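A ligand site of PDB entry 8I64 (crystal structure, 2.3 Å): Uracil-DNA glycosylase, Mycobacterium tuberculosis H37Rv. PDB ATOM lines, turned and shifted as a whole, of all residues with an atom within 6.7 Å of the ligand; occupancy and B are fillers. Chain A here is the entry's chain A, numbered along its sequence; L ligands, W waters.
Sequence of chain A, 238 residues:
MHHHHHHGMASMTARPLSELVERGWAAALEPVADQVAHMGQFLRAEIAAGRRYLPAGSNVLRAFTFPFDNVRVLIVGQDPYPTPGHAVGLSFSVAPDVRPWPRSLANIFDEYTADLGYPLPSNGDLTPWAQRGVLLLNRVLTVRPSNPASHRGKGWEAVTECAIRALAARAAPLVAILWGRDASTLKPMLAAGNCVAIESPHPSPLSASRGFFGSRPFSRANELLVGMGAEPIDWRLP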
ATOM      1  N   VAL A  76     -25.663   7.121  21.659  1.00  0.00           N
ATOM      2  CA  VAL A  76     -24.359   6.485  21.316  1.00  0.00           C
ATOM      3  C   VAL A  76     -23.251   7.315  21.937  1.00  0.00           C
ATOM      4  O   VAL A  76     -23.099   8.495  21.553  1.00  0.00           O
ATOM      5  CB  VAL A  76     -24.127   6.310  19.794  1.00  0.00           C
ATOM      6  CG1 VAL A  76     -22.967   5.364  19.547  1.00  0.00           C
ATOM      7  CG2 VAL A  76     -25.373   5.807  19.080  1.00  0.00           C
ATOM      8  N   GLY A  77     -22.499   6.685  22.847  1.00  0.00           N
ATOM      9  CA  GLY A  77     -21.248   7.224  23.394  1.00  0.00           C
ATOM     10  C   GLY A  77     -20.047   6.613  22.707  1.00  0.00           C
ATOM     11  O   GLY A  77     -20.179   6.088  21.575  1.00  0.00           O
ATOM     12  N   GLN A  78     -18.909   6.691  23.391  1.00  0.00           N
ATOM     13  CA  GLN A  78     -17.581   6.301  22.881  1.00  0.00           C
ATOM     14  C   GLN A  78     -17.207   4.959  23.537  1.00  0.00           C
ATOM     15  O   GLN A  78     -17.320   3.891  22.868  1.00  0.00           O
ATOM     16  CB  GLN A  78     -16.632   7.473  23.166  1.00  0.00           C
ATOM     17  CG  GLN A  78     -17.056   8.793  22.512  1.00  0.00           C
ATOM     18  CD  GLN A  78     -16.192   9.988  22.872  1.00  0.00           C
ATOM     19  OE1 GLN A  78     -16.444  11.128  22.480  1.00  0.00           O
ATOM     20  NE2 GLN A  78     -15.156   9.747  23.650  1.00  0.00           N
ATOM     21  N   ASP A  79     -16.830   5.001  24.824  1.00  0.00           N
ATOM     22  CA  ASP A  79     -16.232   3.849  25.549  1.00  0.00           C
ATOM     23  C   ASP A  79     -16.775   3.760  26.973  1.00  0.00           C
ATOM     24  O   ASP A  79     -17.124   4.788  27.566  1.00  0.00           O
ATOM     25  CB  ASP A  79     -14.703   3.974  25.603  1.00  0.00           C
ATOM     26  CG  ASP A  79     -14.108   4.114  24.229  1.00  0.00           C
ATOM     27  OD1 ASP A  79     -14.219   5.207  23.654  1.00  0.00           O
ATOM     28  OD2 ASP A  79     -13.558   3.114  23.738  1.00  0.00           O
ATOM     29  N   PRO A  80     -16.820   2.539  27.555  1.00  0.00           N
ATOM     30  CA  PRO A  80     -17.236   2.369  28.934  1.00  0.00           C
ATOM     31  C   PRO A  80     -16.351   3.187  29.882  1.00  0.00           C
ATOM     32  O   PRO A  80     -15.238   3.525  29.502  1.00  0.00           O
ATOM     33  CB  PRO A  80     -17.084   0.867  29.181  1.00  0.00           C
ATOM     34  CG  PRO A  80     -17.117   0.253  27.815  1.00  0.00           C
ATOM     35  CD  PRO A  80     -16.482   1.273  26.909  1.00  0.00           C
ATOM     36  N   TYR A  81     -16.922   3.576  31.031  1.00  0.00           N
ATOM     37  CA  TYR A  81     -16.226   4.230  32.172  1.00  0.00           C
ATOM     38  C   TYR A  81     -14.987   3.392  32.484  1.00  0.00           C
ATOM     39  O   TYR A  81     -15.111   2.189  32.653  1.00  0.00           O
ATOM     40  CB  TYR A  81     -17.152   4.288  33.388  1.00  0.00           C
ATOM     41  CG  TYR A  81     -18.271   5.314  33.378  1.00  0.00           C
ATOM     42  CD1 TYR A  81     -18.008   6.673  33.258  1.00  0.00           C
ATOM     43  CD2 TYR A  81     -19.595   4.941  33.576  1.00  0.00           C
ATOM     44  CE1 TYR A  81     -19.035   7.613  33.263  1.00  0.00           C
ATOM     45  CE2 TYR A  81     -20.630   5.860  33.583  1.00  0.00           C
ATOM     46  CZ  TYR A  81     -20.350   7.210  33.448  1.00  0.00           C
ATOM     47  OH  TYR A  81     -21.349   8.131  33.477  1.00  0.00           O
ATOM     48  N   PRO A  82     -13.756   3.973  32.531  1.00  0.00           N
ATOM     49  CA  PRO A  82     -12.563   3.183  32.836  1.00  0.00           C
ATOM     50  C   PRO A  82     -12.309   2.853  34.326  1.00  0.00           C
ATOM     51  O   PRO A  82     -11.500   1.995  34.575  1.00  0.00           O
ATOM     52  CB  PRO A  82     -11.394   4.000  32.262  1.00  0.00           C
ATOM     53  CG  PRO A  82     -11.935   5.420  32.095  1.00  0.00           C
ATOM     54  CD  PRO A  82     -13.446   5.371  32.203  1.00  0.00           C
ATOM     55  N   ALA A  87     -18.702   1.316  35.115  1.00  0.00           N
ATOM     56  CA  ALA A  87     -19.286   0.649  33.925  1.00  0.00           C
ATOM     57  C   ALA A  87     -20.259  -0.473  34.308  1.00  0.00           C
ATOM     58  O   ALA A  87     -19.834  -1.364  35.062  1.00  0.00           O
ATOM     59  CB  ALA A  87     -18.181   0.129  33.047  1.00  0.00           C
ATOM     60  N   LEU A  90     -24.686  -0.451  30.303  1.00  0.00           N
ATOM     61  CA  LEU A  90     -25.564   0.603  29.754  1.00  0.00           C
ATOM     62  C   LEU A  90     -24.754   1.906  29.736  1.00  0.00           C
ATOM     63  O   LEU A  90     -24.276   2.290  30.816  1.00  0.00           O
ATOM     64  CB  LEU A  90     -26.824   0.734  30.625  1.00  0.00           C
ATOM     65  CG  LEU A  90     -27.794  -0.447  30.655  1.00  0.00           C
ATOM     66  CD1 LEU A  90     -28.886  -0.191  31.681  1.00  0.00           C
ATOM     67  CD2 LEU A  90     -28.426  -0.720  29.287  1.00  0.00           C
ATOM     68  N   SER A  91     -24.559   2.541  28.568  1.00  0.00           N
ATOM     69  CA  SER A  91     -23.721   3.758  28.438  1.00  0.00           C
ATOM     70  C   SER A  91     -24.149   4.778  29.518  1.00  0.00           C
ATOM     71  O   SER A  91     -25.372   4.982  29.678  1.00  0.00           O
ATOM     72  CB  SER A  91     -23.720   4.330  27.030  1.00  0.00           C
ATOM     73  OG  SER A  91     -25.009   4.758  26.590  1.00  0.00           O
ATOM     74  N   PHE A  92     -23.185   5.274  30.306  1.00  0.00           N
ATOM     75  CA  PHE A  92     -23.284   6.434  31.250  1.00  0.00           C
ATOM     76  C   PHE A  92     -23.889   6.024  32.603  1.00  0.00           C
ATOM     77  O   PHE A  92     -23.745   6.804  33.601  1.00  0.00           O
ATOM     78  CB  PHE A  92     -24.021   7.608  30.593  1.00  0.00           C
ATOM     79  CG  PHE A  92     -23.282   8.081  29.372  1.00  0.00           C
ATOM     80  CD1 PHE A  92     -22.132   8.846  29.505  1.00  0.00           C
ATOM     81  CD2 PHE A  92     -23.667   7.688  28.092  1.00  0.00           C
ATOM     82  CE1 PHE A  92     -21.400   9.256  28.399  1.00  0.00           C
ATOM     83  CE2 PHE A  92     -22.935   8.087  26.985  1.00  0.00           C
ATOM     84  CZ  PHE A  92     -21.812   8.871  27.136  1.00  0.00           C
ATOM     85  N   SER A  93     -24.557   4.878  32.647  1.00  0.00           N
ATOM     86  CA  SER A  93     -25.200   4.329  33.862  1.00  0.00           C
ATOM     87  C   SER A  93     -24.150   3.872  34.882  1.00  0.00           C
ATOM     88  O   SER A  93     -23.031   3.460  34.478  1.00  0.00           O
ATOM     89  CB  SER A  93     -26.138   3.210  33.513  1.00  0.00           C
ATOM     90  OG  SER A  93     -26.859   2.830  34.669  1.00  0.00           O
ATOM     91  N   PRO A 102     -19.759   9.528  38.189  1.00  0.00           N
ATOM     92  CA  PRO A 102     -18.788   9.917  37.163  1.00  0.00           C
ATOM     93  C   PRO A 102     -19.162  11.278  36.549  1.00  0.00           C
ATOM     94  O   PRO A 102     -20.318  11.632  36.486  1.00  0.00           O
ATOM     95  CB  PRO A 102     -18.879   8.811  36.095  1.00  0.00           C
ATOM     96  CG  PRO A 102     -19.632   7.662  36.761  1.00  0.00           C
ATOM     97  CD  PRO A 102     -20.468   8.290  37.859  1.00  0.00           C
ATOM     98  N   SER A 104     -19.208  12.515  33.529  1.00  0.00           N
ATOM     99  CA  SER A 104     -20.109  12.503  32.339  1.00  0.00           C
ATOM    100  C   SER A 104     -21.572  12.466  32.796  1.00  0.00           C
ATOM    101  O   SER A 104     -22.415  13.211  32.233  1.00  0.00           O
ATOM    102  CB  SER A 104     -19.766  11.365  31.424  1.00  0.00           C
ATOM    103  OG  SER A 104     -18.664  11.734  30.613  1.00  0.00           O
ATOM    104  N   LEU A 105     -21.856  11.641  33.819  1.00  0.00           N
ATOM    105  CA  LEU A 105     -23.237  11.447  34.314  1.00  0.00           C
ATOM    106  C   LEU A 105     -23.678  12.726  35.050  1.00  0.00           C
ATOM    107  O   LEU A 105     -24.787  13.138  34.820  1.00  0.00           O
ATOM    108  CB  LEU A 105     -23.294  10.187  35.199  1.00  0.00           C
ATOM    109  CG  LEU A 105     -24.691   9.705  35.570  1.00  0.00           C
ATOM    110  CD1 LEU A 105     -25.574   9.465  34.361  1.00  0.00           C
ATOM    111  CD2 LEU A 105     -24.634   8.432  36.414  1.00  0.00           C
ATOM    112  N   LEU A 137     -25.997   3.015  24.176  1.00  0.00           N
ATOM    113  CA  LEU A 137     -24.951   2.288  23.424  1.00  0.00           C
ATOM    114  C   LEU A 137     -23.638   3.042  23.545  1.00  0.00           C
ATOM    115  O   LEU A 137     -23.679   4.269  23.657  1.00  0.00           O
ATOM    116  CB  LEU A 137     -25.397   2.147  21.967  1.00  0.00           C
ATOM    117  CG  LEU A 137     -24.531   1.213  21.115  1.00  0.00           C
ATOM    118  CD1 LEU A 137     -24.519  -0.186  21.721  1.00  0.00           C
ATOM    119  CD2 LEU A 137     -25.029   1.179  19.683  1.00  0.00           C
ATOM    120  N   ASN A 138     -22.543   2.295  23.566  1.00  0.00           N
ATOM    121  CA  ASN A 138     -21.173   2.820  23.379  1.00  0.00           C
ATOM    122  C   ASN A 138     -20.708   2.221  22.058  1.00  0.00           C
ATOM    123  O   ASN A 138     -21.047   1.049  21.809  1.00  0.00           O
ATOM    124  CB  ASN A 138     -20.264   2.502  24.562  1.00  0.00           C
ATOM    125  CG  ASN A 138     -20.406   3.453  25.731  1.00  0.00           C
ATOM    126  OD1 ASN A 138     -20.349   4.673  25.549  1.00  0.00           O
ATOM    127  ND2 ASN A 138     -20.611   2.907  26.924  1.00  0.00           N
ATOM    128  N   TRP A 179     -23.333  11.605  20.991  1.00  0.00           N
ATOM    129  CA  TRP A 179     -22.470  12.322  21.954  1.00  0.00           C
ATOM    130  C   TRP A 179     -21.015  11.994  21.628  1.00  0.00           C
ATOM    131  O   TRP A 179     -20.647  10.806  21.782  1.00  0.00           O
ATOM    132  CB  TRP A 179     -22.846  11.951  23.402  1.00  0.00           C
ATOM    133  CG  TRP A 179     -24.147  12.513  23.856  1.00  0.00           C
ATOM    134  CD1 TRP A 179     -24.797  13.578  23.309  1.00  0.00           C
ATOM    135  CD2 TRP A 179     -24.944  12.110  24.990  1.00  0.00           C
ATOM    136  NE1 TRP A 179     -25.932  13.851  24.016  1.00  0.00           N
ATOM    137  CE2 TRP A 179     -26.047  12.984  25.046  1.00  0.00           C
ATOM    138  CE3 TRP A 179     -24.841  11.106  25.951  1.00  0.00           C
ATOM    139  CZ2 TRP A 179     -27.074  12.865  25.997  1.00  0.00           C
ATOM    140  CZ3 TRP A 179     -25.837  10.978  26.904  1.00  0.00           C
ATOM    141  CH2 TRP A 179     -26.925  11.854  26.935  1.00  0.00           C
ATOM    142  N   HIS A 202     -19.379  15.680  23.468  1.00  0.00           N
ATOM    143  CA  HIS A 202     -19.504  14.651  24.539  1.00  0.00           C
ATOM    144  C   HIS A 202     -19.734  15.352  25.872  1.00  0.00           C
ATOM    145  O   HIS A 202     -19.120  16.377  26.151  1.00  0.00           O
ATOM    146  CB  HIS A 202     -18.230  13.772  24.584  1.00  0.00           C
ATOM    147  CG  HIS A 202     -18.378  12.482  25.316  1.00  0.00           C
ATOM    148  ND1 HIS A 202     -18.258  12.398  26.700  1.00  0.00           N
ATOM    149  CD2 HIS A 202     -18.576  11.222  24.873  1.00  0.00           C
ATOM    150  CE1 HIS A 202     -18.406  11.138  27.082  1.00  0.00           C
ATOM    151  NE2 HIS A 202     -18.592  10.399  25.971  1.00  0.00           N
ATOM    152  N   PRO A 203     -20.573  14.803  26.777  1.00  0.00           N
ATOM    153  CA  PRO A 203     -20.777  15.396  28.102  1.00  0.00           C
ATOM    154  C   PRO A 203     -19.585  15.328  29.080  1.00  0.00           C
ATOM    155  O   PRO A 203     -19.729  15.780  30.170  1.00  0.00           O
ATOM    156  CB  PRO A 203     -21.887  14.512  28.691  1.00  0.00           C
ATOM    157  CG  PRO A 203     -21.655  13.190  28.020  1.00  0.00           C
ATOM    158  CD  PRO A 203     -21.335  13.568  26.597  1.00  0.00           C
ATOM    159  N   SER A 204     -18.462  14.776  28.662  1.00  0.00           N
ATOM    160  CA  SER A 204     -17.200  14.727  29.436  1.00  0.00           C
ATOM    161  C   SER A 204     -16.710  16.146  29.722  1.00  0.00           C
ATOM    162  O   SER A 204     -16.916  17.050  28.901  1.00  0.00           O
ATOM    163  CB  SER A 204     -16.183  13.858  28.700  1.00  0.00           C
ATOM    164  OG  SER A 204     -14.846  14.205  29.057  1.00  0.00           O
HETATM  165  N1  LIG L   1     -19.732   6.186  27.643  1.00  0.00           N
HETATM  166  C1  LIG L   1     -18.872   7.192  27.277  1.00  0.00           C
HETATM  167  O1  LIG L   1     -18.642   7.437  26.114  1.00  0.00           O
HETATM  168  N2  LIG L   1     -18.239   7.866  28.300  1.00  0.00           N
HETATM  169  C2  LIG L   1     -18.224   7.488  29.614  1.00  0.00           C
HETATM  170  O2  LIG L   1     -17.606   8.126  30.454  1.00  0.00           O
HETATM  171  C3  LIG L   1     -19.040   6.284  29.986  1.00  0.00           C
HETATM  172  C4  LIG L   1     -19.849   5.664  28.897  1.00  0.00           C
HETATM  173  O3  LIG L   1     -20.611   4.738  29.104  1.00  0.00           O
HETATM  174  O   HOH W   1     -20.028   2.620  30.976  1.00  0.00           O
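N1 of the ligand lies within hydrogen-bond range of OD1 of Asn 138. O of Asp 79 lies within hydrogen-bond range of N1 of the ligand (3.0 Å). An oxygen (O1) of the ligand sits at hydrogen-bond distance from the backbone NH (N) of Gln 78, at 2.8 Å. The backbone NH of Phe 92 lies within hydrogen-bond range of an oxygen (O3) of the ligand, at 2.9 Å. NE2 of His 202 sits at hydrogen-bond distance from O1 of the ligand, at 3.0 Å. N of Asp 79 lies within hydrogen-bond range of O1 of the ligand (3.3 Å).
The backbone NH (N) of Gln 78 lies within hydrogen-bond range of the side-chain amide oxygen (OD1) of Asn 138 (3.3 Å). ND1 of His 202 sits at hydrogen-bond distance from N of Ser 204, 3.1 Å away. The backbone carbonyl oxygen (O) of Leu 137 is in hydrogen-bond range of the backbone NH (N) of Gly 77, at 2.8 Å. The backbone carbonyl oxygen of Phe 92 sits at hydrogen-bond distance from the side-chain hydroxyl of Tyr 81, 2.7 Å away. The side-chain hydroxyl (OG) of Ser 91 is in hydrogen-bond range of the backbone NH (N) of Leu 137 (3.1 Å).
Gly 77 touches the ligand (CA to O1, 3.8 Å). Tyr 81 touches the ligand. Ser 91 touches the ligand (CA to O3, 3.3 Å). OG of Ser 104 touches O2 of the ligand, at 3.8 Å.
Water W1 lies within hydrogen-bond range of an oxygen (O3) of the ligand and the backbone NH (N) of Tyr 81.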
